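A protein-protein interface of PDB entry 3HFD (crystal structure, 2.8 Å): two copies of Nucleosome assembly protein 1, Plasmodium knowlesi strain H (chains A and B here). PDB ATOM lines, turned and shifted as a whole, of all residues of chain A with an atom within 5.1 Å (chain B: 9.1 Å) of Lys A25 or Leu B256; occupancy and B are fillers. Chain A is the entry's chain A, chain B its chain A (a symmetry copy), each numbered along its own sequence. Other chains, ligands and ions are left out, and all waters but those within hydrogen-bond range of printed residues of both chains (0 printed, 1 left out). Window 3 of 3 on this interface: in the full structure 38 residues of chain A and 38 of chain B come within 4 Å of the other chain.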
ATOM      1  N   LEU A  21      22.665  -9.447  26.244  1.00  0.00           N
ATOM      2  CA  LEU A  21      21.800  -8.490  25.569  1.00  0.00           C
ATOM      3  C   LEU A  21      20.399  -9.058  25.340  1.00  0.00           C
ATOM      4  O   LEU A  21      19.414  -8.376  25.581  1.00  0.00           O
ATOM      5  CB  LEU A  21      22.428  -8.048  24.251  1.00  0.00           C
ATOM      6  CG  LEU A  21      22.350  -6.563  23.932  1.00  0.00           C
ATOM      7  CD1 LEU A  21      22.711  -5.697  25.131  1.00  0.00           C
ATOM      8  CD2 LEU A  21      23.294  -6.295  22.779  1.00  0.00           C
ATOM      9  N   LYS A  22      20.302 -10.300  24.882  1.00  0.00           N
ATOM     10  CA  LYS A  22      19.001 -10.963  24.859  1.00  0.00           C
ATOM     11  C   LYS A  22      18.298 -10.708  26.179  1.00  0.00           C
ATOM     12  O   LYS A  22      17.198 -10.166  26.213  1.00  0.00           O
ATOM     13  CB  LYS A  22      19.119 -12.475  24.642  1.00  0.00           C
ATOM     14  CG  LYS A  22      18.624 -12.916  23.310  1.00  0.00           C
ATOM     15  CD  LYS A  22      18.632 -14.425  23.172  1.00  0.00           C
ATOM     16  CE  LYS A  22      17.284 -15.062  23.455  1.00  0.00           C
ATOM     17  NZ  LYS A  22      17.372 -16.525  23.189  1.00  0.00           N
ATOM     18  N   LYS A  23      18.945 -11.094  27.270  1.00  0.00           N
ATOM     19  CA  LYS A  23      18.337 -10.956  28.581  1.00  0.00           C
ATOM     20  C   LYS A  23      17.892  -9.507  28.815  1.00  0.00           C
ATOM     21  O   LYS A  23      16.764  -9.258  29.234  1.00  0.00           O
ATOM     22  CB  LYS A  23      19.302 -11.442  29.669  1.00  0.00           C
ATOM     23  CG  LYS A  23      19.291 -12.968  29.852  1.00  0.00           C
ATOM     24  CD  LYS A  23      20.609 -13.515  30.419  1.00  0.00           C
ATOM     25  CE  LYS A  23      20.846 -13.076  31.869  1.00  0.00           C
ATOM     26  NZ  LYS A  23      22.259 -13.285  32.312  1.00  0.00           N
ATOM     27  N   LEU A  24      18.767  -8.557  28.499  1.00  0.00           N
ATOM     28  CA  LEU A  24      18.453  -7.140  28.672  1.00  0.00           C
ATOM     29  C   LEU A  24      17.295  -6.707  27.788  1.00  0.00           C
ATOM     30  O   LEU A  24      16.393  -6.012  28.253  1.00  0.00           O
ATOM     31  CB  LEU A  24      19.683  -6.259  28.413  1.00  0.00           C
ATOM     32  CG  LEU A  24      20.519  -5.922  29.653  1.00  0.00           C
ATOM     33  CD1 LEU A  24      20.657  -7.128  30.554  1.00  0.00           C
ATOM     34  CD2 LEU A  24      21.901  -5.371  29.273  1.00  0.00           C
ATOM     35  N   LYS A  25      17.320  -7.114  26.522  1.00  0.00           N
ATOM     36  CA  LYS A  25      16.224  -6.822  25.604  1.00  0.00           C
ATOM     37  C   LYS A  25      14.946  -7.427  26.172  1.00  0.00           C
ATOM     38  O   LYS A  25      13.878  -6.824  26.095  1.00  0.00           O
ATOM     39  CB  LYS A  25      16.484  -7.403  24.205  1.00  0.00           C
ATOM     40  CG  LYS A  25      17.672  -6.794  23.439  1.00  0.00           C
ATOM     41  CD  LYS A  25      17.260  -5.634  22.534  1.00  0.00           C
ATOM     42  CE  LYS A  25      16.880  -6.094  21.105  1.00  0.00           C
ATOM     43  NZ  LYS A  25      15.887  -5.160  20.410  1.00  0.00           N
ATOM     44  N   LEU A  26      15.065  -8.609  26.765  1.00  0.00           N
ATOM     45  CA  LEU A  26      13.912  -9.292  27.332  1.00  0.00           C
ATOM     46  C   LEU A  26      13.301  -8.507  28.487  1.00  0.00           C
ATOM     47  O   LEU A  26      12.108  -8.236  28.495  1.00  0.00           O
ATOM     48  CB  LEU A  26      14.299 -10.693  27.805  1.00  0.00           C
ATOM     49  CG  LEU A  26      13.109 -11.535  28.252  1.00  0.00           C
ATOM     50  CD1 LEU A  26      12.234 -11.847  27.038  1.00  0.00           C
ATOM     51  CD2 LEU A  26      13.575 -12.804  28.973  1.00  0.00           C
ATOM     52  N   TYR A  27      14.131  -8.143  29.453  1.00  0.00           N
ATOM     53  CA  TYR A  27      13.679  -7.408  30.628  1.00  0.00           C
ATOM     54  C   TYR A  27      13.141  -6.028  30.295  1.00  0.00           C
ATOM     55  O   TYR A  27      12.288  -5.513  31.004  1.00  0.00           O
ATOM     56  CB  TYR A  27      14.822  -7.234  31.607  1.00  0.00           C
ATOM     57  CG  TYR A  27      15.589  -8.488  31.916  1.00  0.00           C
ATOM     58  CD1 TYR A  27      14.950  -9.720  32.018  1.00  0.00           C
ATOM     59  CD2 TYR A  27      16.959  -8.434  32.132  1.00  0.00           C
ATOM     60  CE1 TYR A  27      15.662 -10.866  32.313  1.00  0.00           C
ATOM     61  CE2 TYR A  27      17.679  -9.566  32.427  1.00  0.00           C
ATOM     62  CZ  TYR A  27      17.029 -10.784  32.519  1.00  0.00           C
ATOM     63  OH  TYR A  27      17.764 -11.915  32.817  1.00  0.00           O
ATOM     64  N   GLN A  28      13.666  -5.424  29.234  1.00  0.00           N
ATOM     65  CA  GLN A  28      13.249  -4.084  28.803  1.00  0.00           C
ATOM     66  C   GLN A  28      11.924  -4.153  28.067  1.00  0.00           C
ATOM     67  O   GLN A  28      11.251  -3.142  27.897  1.00  0.00           O
ATOM     68  CB  GLN A  28      14.320  -3.457  27.899  1.00  0.00           C
ATOM     69  CG  GLN A  28      14.108  -2.006  27.542  1.00  0.00           C
ATOM     70  CD  GLN A  28      13.882  -1.140  28.753  1.00  0.00           C
ATOM     71  OE1 GLN A  28      12.812  -0.556  28.908  1.00  0.00           O
ATOM     72  NE2 GLN A  28      14.879  -1.066  29.638  1.00  0.00           N
ATOM     73  N   LYS A  29      11.561  -5.346  27.610  1.00  0.00           N
ATOM     74  CA  LYS A  29      10.256  -5.572  27.001  1.00  0.00           C
ATOM     75  C   LYS A  29       9.229  -5.674  28.116  1.00  0.00           C
ATOM     76  O   LYS A  29       8.174  -5.027  28.072  1.00  0.00           O
ATOM     77  CB  LYS A  29      10.254  -6.857  26.163  1.00  0.00           C
ATOM     78  CG  LYS A  29       9.071  -6.982  25.215  1.00  0.00           C
ATOM     79  CD  LYS A  29       9.154  -5.977  24.058  1.00  0.00           C
ATOM     80  CE  LYS A  29       8.328  -4.703  24.285  1.00  0.00           C
ATOM     81  NZ  LYS A  29       8.891  -3.544  23.514  1.00  0.00           N
ATOM     82  N   ILE B  56      12.791  -6.275  37.727  1.00  0.00           N
ATOM     83  CA  ILE B  56      13.293  -6.117  36.365  1.00  0.00           C
ATOM     84  C   ILE B  56      14.664  -5.439  36.371  1.00  0.00           C
ATOM     85  O   ILE B  56      15.594  -5.911  35.718  1.00  0.00           O
ATOM     86  CB  ILE B  56      12.335  -5.277  35.510  1.00  0.00           C
ATOM     87  CG1 ILE B  56      11.005  -6.010  35.336  1.00  0.00           C
ATOM     88  CG2 ILE B  56      12.992  -4.944  34.169  1.00  0.00           C
ATOM     89  CD1 ILE B  56      10.015  -5.251  34.484  1.00  0.00           C
ATOM     90  N   ARG B  60      18.225  -7.109  35.419  1.00  0.00           N
ATOM     91  CA  ARG B  60      19.119  -6.473  34.462  1.00  0.00           C
ATOM     92  C   ARG B  60      20.498  -6.269  35.075  1.00  0.00           C
ATOM     93  O   ARG B  60      21.509  -6.481  34.405  1.00  0.00           O
ATOM     94  CB  ARG B  60      18.530  -5.156  33.982  1.00  0.00           C
ATOM     95  CG  ARG B  60      19.550  -4.119  33.541  1.00  0.00           C
ATOM     96  CD  ARG B  60      19.121  -2.722  34.007  1.00  0.00           C
ATOM     97  NE  ARG B  60      18.280  -2.048  33.030  1.00  0.00           N
ATOM     98  CZ  ARG B  60      17.666  -0.888  33.240  1.00  0.00           C
ATOM     99  NH1 ARG B  60      17.759  -0.259  34.418  1.00  0.00           N
ATOM    100  NH2 ARG B  60      16.942  -0.356  32.251  1.00  0.00           N
ATOM    101  N   ALA B  63      22.263  -9.535  35.107  1.00  0.00           N
ATOM    102  CA  ALA B  63      22.787  -9.895  33.796  1.00  0.00           C
ATOM    103  C   ALA B  63      24.077  -9.155  33.451  1.00  0.00           C
ATOM    104  O   ALA B  63      24.963  -9.732  32.831  1.00  0.00           O
ATOM    105  CB  ALA B  63      21.746  -9.661  32.725  1.00  0.00           C
ATOM    106  N   LEU B  77      28.755  -7.009  30.071  1.00  0.00           N
ATOM    107  CA  LEU B  77      28.495  -6.136  28.933  1.00  0.00           C
ATOM    108  C   LEU B  77      29.279  -4.850  29.202  1.00  0.00           C
ATOM    109  O   LEU B  77      28.749  -3.871  29.734  1.00  0.00           O
ATOM    110  CB  LEU B  77      26.991  -5.882  28.789  1.00  0.00           C
ATOM    111  CG  LEU B  77      26.474  -5.291  27.480  1.00  0.00           C
ATOM    112  CD1 LEU B  77      26.800  -6.230  26.336  1.00  0.00           C
ATOM    113  CD2 LEU B  77      24.949  -5.031  27.585  1.00  0.00           C
ATOM    114  N   GLU B  79      31.174  -1.406  29.623  1.00  0.00           N
ATOM    115  CA  GLU B  79      30.880  -0.005  29.300  1.00  0.00           C
ATOM    116  C   GLU B  79      29.396   0.269  29.002  1.00  0.00           C
ATOM    117  O   GLU B  79      29.066   1.185  28.245  1.00  0.00           O
ATOM    118  CB  GLU B  79      31.770   0.474  28.143  1.00  0.00           C
ATOM    119  CG  GLU B  79      33.218  -0.002  28.253  1.00  0.00           C
ATOM    120  CD  GLU B  79      34.202   0.774  27.379  1.00  0.00           C
ATOM    121  OE1 GLU B  79      33.772   1.602  26.542  1.00  0.00           O
ATOM    122  OE2 GLU B  79      35.424   0.544  27.537  1.00  0.00           O
ATOM    123  N   PHE B  80      28.509  -0.507  29.630  1.00  0.00           N
ATOM    124  CA  PHE B  80      27.056  -0.429  29.372  1.00  0.00           C
ATOM    125  C   PHE B  80      26.458   0.907  29.813  1.00  0.00           C
ATOM    126  O   PHE B  80      25.766   1.586  29.054  1.00  0.00           O
ATOM    127  CB  PHE B  80      26.319  -1.587  30.083  1.00  0.00           C
ATOM    128  CG  PHE B  80      24.806  -1.506  29.992  1.00  0.00           C
ATOM    129  CD1 PHE B  80      24.140  -1.974  28.881  1.00  0.00           C
ATOM    130  CD2 PHE B  80      24.064  -0.968  31.017  1.00  0.00           C
ATOM    131  CE1 PHE B  80      22.781  -1.904  28.803  1.00  0.00           C
ATOM    132  CE2 PHE B  80      22.688  -0.902  30.939  1.00  0.00           C
ATOM    133  CZ  PHE B  80      22.052  -1.368  29.844  1.00  0.00           C
ATOM    134  N   ARG B  83      28.087   4.092  28.088  1.00  0.00           N
ATOM    135  CA  ARG B  83      27.574   4.249  26.731  1.00  0.00           C
ATOM    136  C   ARG B  83      26.086   4.583  26.676  1.00  0.00           C
ATOM    137  O   ARG B  83      25.663   5.353  25.817  1.00  0.00           O
ATOM    138  CB  ARG B  83      27.939   3.035  25.869  1.00  0.00           C
ATOM    139  CG  ARG B  83      29.415   3.101  25.457  1.00  0.00           C
ATOM    140  CD  ARG B  83      29.904   1.932  24.614  1.00  0.00           C
ATOM    141  NE  ARG B  83      30.762   2.412  23.518  1.00  0.00           N
ATOM    142  CZ  ARG B  83      31.829   1.782  23.017  1.00  0.00           C
ATOM    143  NH1 ARG B  83      32.242   0.613  23.507  1.00  0.00           N
ATOM    144  NH2 ARG B  83      32.500   2.345  22.011  1.00  0.00           N
ATOM    145  N   ALA B  84      25.304   4.029  27.599  1.00  0.00           N
ATOM    146  CA  ALA B  84      23.886   4.380  27.719  1.00  0.00           C
ATOM    147  C   ALA B  84      23.704   5.841  28.149  1.00  0.00           C
ATOM    148  O   ALA B  84      22.848   6.534  27.623  1.00  0.00           O
ATOM    149  CB  ALA B  84      23.178   3.443  28.691  1.00  0.00           C
ATOM    150  N   LEU B  85      24.507   6.300  29.105  1.00  0.00           N
ATOM    151  CA  LEU B  85      24.552   7.729  29.482  1.00  0.00           C
ATOM    152  C   LEU B  85      24.977   8.639  28.314  1.00  0.00           C
ATOM    153  O   LEU B  85      24.436   9.728  28.148  1.00  0.00           O
ATOM    154  CB  LEU B  85      25.522   7.967  30.646  1.00  0.00           C
ATOM    155  CG  LEU B  85      25.320   7.288  32.005  1.00  0.00           C
ATOM    156  CD1 LEU B  85      26.509   7.603  32.920  1.00  0.00           C
ATOM    157  CD2 LEU B  85      24.005   7.721  32.641  1.00  0.00           C
ATOM    158  N   ASN B  87      24.556   8.303  25.125  1.00  0.00           N
ATOM    159  CA  ASN B  87      23.504   8.434  24.098  1.00  0.00           C
ATOM    160  C   ASN B  87      22.279   9.265  24.546  1.00  0.00           C
ATOM    161  O   ASN B  87      21.316   9.395  23.793  1.00  0.00           O
ATOM    162  CB  ASN B  87      23.055   7.050  23.607  1.00  0.00           C
ATOM    163  CG  ASN B  87      24.102   6.362  22.762  1.00  0.00           C
ATOM    164  OD1 ASN B  87      25.237   6.809  22.699  1.00  0.00           O
ATOM    165  ND2 ASN B  87      23.726   5.267  22.112  1.00  0.00           N
ATOM    166  N   TYR B 250      15.005   3.025  30.401  1.00  0.00           N
ATOM    167  CA  TYR B 250      15.256   2.635  29.018  1.00  0.00           C
ATOM    168  C   TYR B 250      16.742   2.453  28.738  1.00  0.00           C
ATOM    169  O   TYR B 250      17.189   2.660  27.612  1.00  0.00           O
ATOM    170  CB  TYR B 250      14.682   3.703  28.091  1.00  0.00           C
ATOM    171  CG  TYR B 250      13.347   4.256  28.562  1.00  0.00           C
ATOM    172  CD1 TYR B 250      12.293   3.413  28.883  1.00  0.00           C
ATOM    173  CD2 TYR B 250      13.146   5.623  28.687  1.00  0.00           C
ATOM    174  CE1 TYR B 250      11.088   3.916  29.319  1.00  0.00           C
ATOM    175  CE2 TYR B 250      11.944   6.137  29.123  1.00  0.00           C
ATOM    176  CZ  TYR B 250      10.920   5.281  29.432  1.00  0.00           C
ATOM    177  OH  TYR B 250       9.721   5.805  29.857  1.00  0.00           O
ATOM    178  N   ALA B 251      17.494   2.036  29.760  1.00  0.00           N
ATOM    179  CA  ALA B 251      18.961   2.012  29.720  1.00  0.00           C
ATOM    180  C   ALA B 251      19.538   1.353  28.474  1.00  0.00           C
ATOM    181  O   ALA B 251      20.337   1.950  27.747  1.00  0.00           O
ATOM    182  CB  ALA B 251      19.497   1.318  30.963  1.00  0.00           C
ATOM    183  N   VAL B 252      19.136   0.110  28.242  1.00  0.00           N
ATOM    184  CA  VAL B 252      19.621  -0.646  27.097  1.00  0.00           C
ATOM    185  C   VAL B 252      19.261   0.031  25.758  1.00  0.00           C
ATOM    186  O   VAL B 252      20.030  -0.051  24.793  1.00  0.00           O
ATOM    187  CB  VAL B 252      19.081  -2.086  27.131  1.00  0.00           C
ATOM    188  CG1 VAL B 252      17.586  -2.110  26.859  1.00  0.00           C
ATOM    189  CG2 VAL B 252      19.814  -2.935  26.129  1.00  0.00           C
ATOM    190  N   ASP B 253      18.106   0.702  25.706  1.00  0.00           N
ATOM    191  CA  ASP B 253      17.654   1.378  24.491  1.00  0.00           C
ATOM    192  C   ASP B 253      18.543   2.569  24.193  1.00  0.00           C
ATOM    193  O   ASP B 253      18.850   2.829  23.036  1.00  0.00           O
ATOM    194  CB  ASP B 253      16.193   1.836  24.605  1.00  0.00           C
ATOM    195  CG  ASP B 253      15.193   0.681  24.518  1.00  0.00           C
ATOM    196  OD1 ASP B 253      15.498  -0.431  25.002  1.00  0.00           O
ATOM    197  OD2 ASP B 253      14.093   0.894  23.970  1.00  0.00           O
ATOM    198  N   TYR B 254      18.946   3.301  25.231  1.00  0.00           N
ATOM    199  CA  TYR B 254      19.977   4.337  25.076  1.00  0.00           C
ATOM    200  C   TYR B 254      21.327   3.696  24.709  1.00  0.00           C
ATOM    201  O   TYR B 254      22.068   4.240  23.893  1.00  0.00           O
ATOM    202  CB  TYR B 254      20.130   5.185  26.347  1.00  0.00           C
ATOM    203  CG  TYR B 254      19.084   6.269  26.522  1.00  0.00           C
ATOM    204  CD1 TYR B 254      19.204   7.488  25.873  1.00  0.00           C
ATOM    205  CD2 TYR B 254      17.985   6.084  27.359  1.00  0.00           C
ATOM    206  CE1 TYR B 254      18.254   8.483  26.042  1.00  0.00           C
ATOM    207  CE2 TYR B 254      17.031   7.080  27.532  1.00  0.00           C
ATOM    208  CZ  TYR B 254      17.174   8.270  26.871  1.00  0.00           C
ATOM    209  OH  TYR B 254      16.230   9.255  27.023  1.00  0.00           O
ATOM    210  N   PHE B 255      21.633   2.541  25.310  1.00  0.00           N
ATOM    211  CA  PHE B 255      22.840   1.775  24.971  1.00  0.00           C
ATOM    212  C   PHE B 255      22.808   1.459  23.488  1.00  0.00           C
ATOM    213  O   PHE B 255      23.649   1.942  22.727  1.00  0.00           O
ATOM    214  CB  PHE B 255      22.930   0.480  25.802  1.00  0.00           C
ATOM    215  CG  PHE B 255      24.054  -0.442  25.396  1.00  0.00           C
ATOM    216  CD1 PHE B 255      25.262  -0.429  26.085  1.00  0.00           C
ATOM    217  CD2 PHE B 255      23.902  -1.332  24.329  1.00  0.00           C
ATOM    218  CE1 PHE B 255      26.309  -1.280  25.712  1.00  0.00           C
ATOM    219  CE2 PHE B 255      24.943  -2.182  23.952  1.00  0.00           C
ATOM    220  CZ  PHE B 255      26.150  -2.151  24.646  1.00  0.00           C
ATOM    221  N   LEU B 256      21.811   0.682  23.076  1.00  0.00           N
ATOM    222  CA  LEU B 256      21.640   0.311  21.671  1.00  0.00           C
ATOM    223  C   LEU B 256      21.614   1.520  20.739  1.00  0.00           C
ATOM    224  O   LEU B 256      21.860   1.381  19.548  1.00  0.00           O
ATOM    225  CB  LEU B 256      20.335  -0.477  21.479  1.00  0.00           C
ATOM    226  CG  LEU B 256      20.233  -1.853  22.138  1.00  0.00           C
ATOM    227  CD1 LEU B 256      18.788  -2.160  22.541  1.00  0.00           C
ATOM    228  CD2 LEU B 256      20.788  -2.890  21.199  1.00  0.00           C
ATOM    229  N   GLY B 257      21.283   2.694  21.271  1.00  0.00           N
ATOM    230  CA  GLY B 257      21.336   3.939  20.495  1.00  0.00           C
ATOM    231  C   GLY B 257      20.095   4.161  19.639  1.00  0.00           C
ATOM    232  O   GLY B 257      20.190   4.469  18.446  1.00  0.00           O
ATOM    233  N   ILE B 258      18.930   4.012  20.266  1.00  0.00           N
ATOM    234  CA  ILE B 258      17.658   4.201  19.584  1.00  0.00           C
ATOM    235  C   ILE B 258      16.713   5.186  20.302  1.00  0.00           C
ATOM    236  O   ILE B 258      15.531   5.263  19.956  1.00  0.00           O
ATOM    237  CB  ILE B 258      16.979   2.841  19.280  1.00  0.00           C
ATOM    238  CG1 ILE B 258      16.806   1.987  20.537  1.00  0.00           C
ATOM    239  CG2 ILE B 258      17.815   2.069  18.258  1.00  0.00           C
ATOM    240  CD1 ILE B 258      16.339   0.560  20.232  1.00  0.00           C
ATOM    241  N   ILE B 259      17.226   5.950  21.274  1.00  0.00           N
ATOM    242  CA  ILE B 259      16.491   7.102  21.817  1.00  0.00           C
ATOM    243  C   ILE B 259      17.356   8.358  21.781  1.00  0.00           C
ATOM    244  O   ILE B 259      17.250   9.173  20.862  1.00  0.00           O
ATOM    245  CB  ILE B 259      15.984   6.884  23.272  1.00  0.00           C
ATOM    246  CG1 ILE B 259      15.240   5.544  23.403  1.00  0.00           C
ATOM    247  CG2 ILE B 259      15.070   8.051  23.697  1.00  0.00           C
ATOM    248  CD1 ILE B 259      14.110   5.541  24.445  1.00  0.00           C
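No position is printed for both chains. Of the 13 pairs that touch across the chains among the printed residues, none has its exchanged pair printed and touching as well.
NE2 of Gln A28 sits close to NH2 of Arg B60, 3.4 Å away.
Printed residues of chain B that touch a printed residue of chain A: Ile B56, Arg B60, Ala B63, Leu B77, Phe B80, Tyr B250, Val B252, Asp B253 and Leu B256. Among the printed residues, 13 pairs touch across the chains.
Leu B256 touches one residue of chain A. Of the printed residues of chain B, Lys A23 touches Ala B63 (3.6 Å). Of the printed residues of chain A, Ala B63 touches Lys A23 (3.6 Å) and Leu A24 (3.5 Å). Of the printed residues of chain A, Ile B56 touches Tyr A27 (3.3 Å). Of the printed residues of chain A, Leu B77 touches Leu A21 (3.4 Å) and Leu A24 (3.5 Å). Leu B85 touches none of the printed residues of chain A. The nearest residue of chain A that does not touch Leu B256 is Leu A21 (4.5 Å). The nearest printed residue of chain A that does not touch Ile B56 is Gln A28 (5.0 Å).
Among the printed residues, pairs that only touch across the chains: Leu A21 with Leu B77 (3.4 Å), Lys A23 with Ala B63 (3.6 Å), Leu A24 with Arg B60 (3.997 Å), Leu A24 with Ala B63 (3.5 Å), Leu A24 with Leu B77 (3.5 Å), Leu A24 with Phe B80 (3.6 Å), Lys A25 with Leu B256 (3.8 Å), Tyr A27 with Ile B56 (3.3 Å), Tyr A27 with Arg B60 (3.7 Å), Gln A28 with Tyr B250 (3.8 Å), Gln A28 with Val B252 (3.5 Å) and Gln A28 with Asp B253 (3.3 Å).
O of Asp B253 lies within hydrogen-bond range of N of Ile B258 (3.0 Å).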
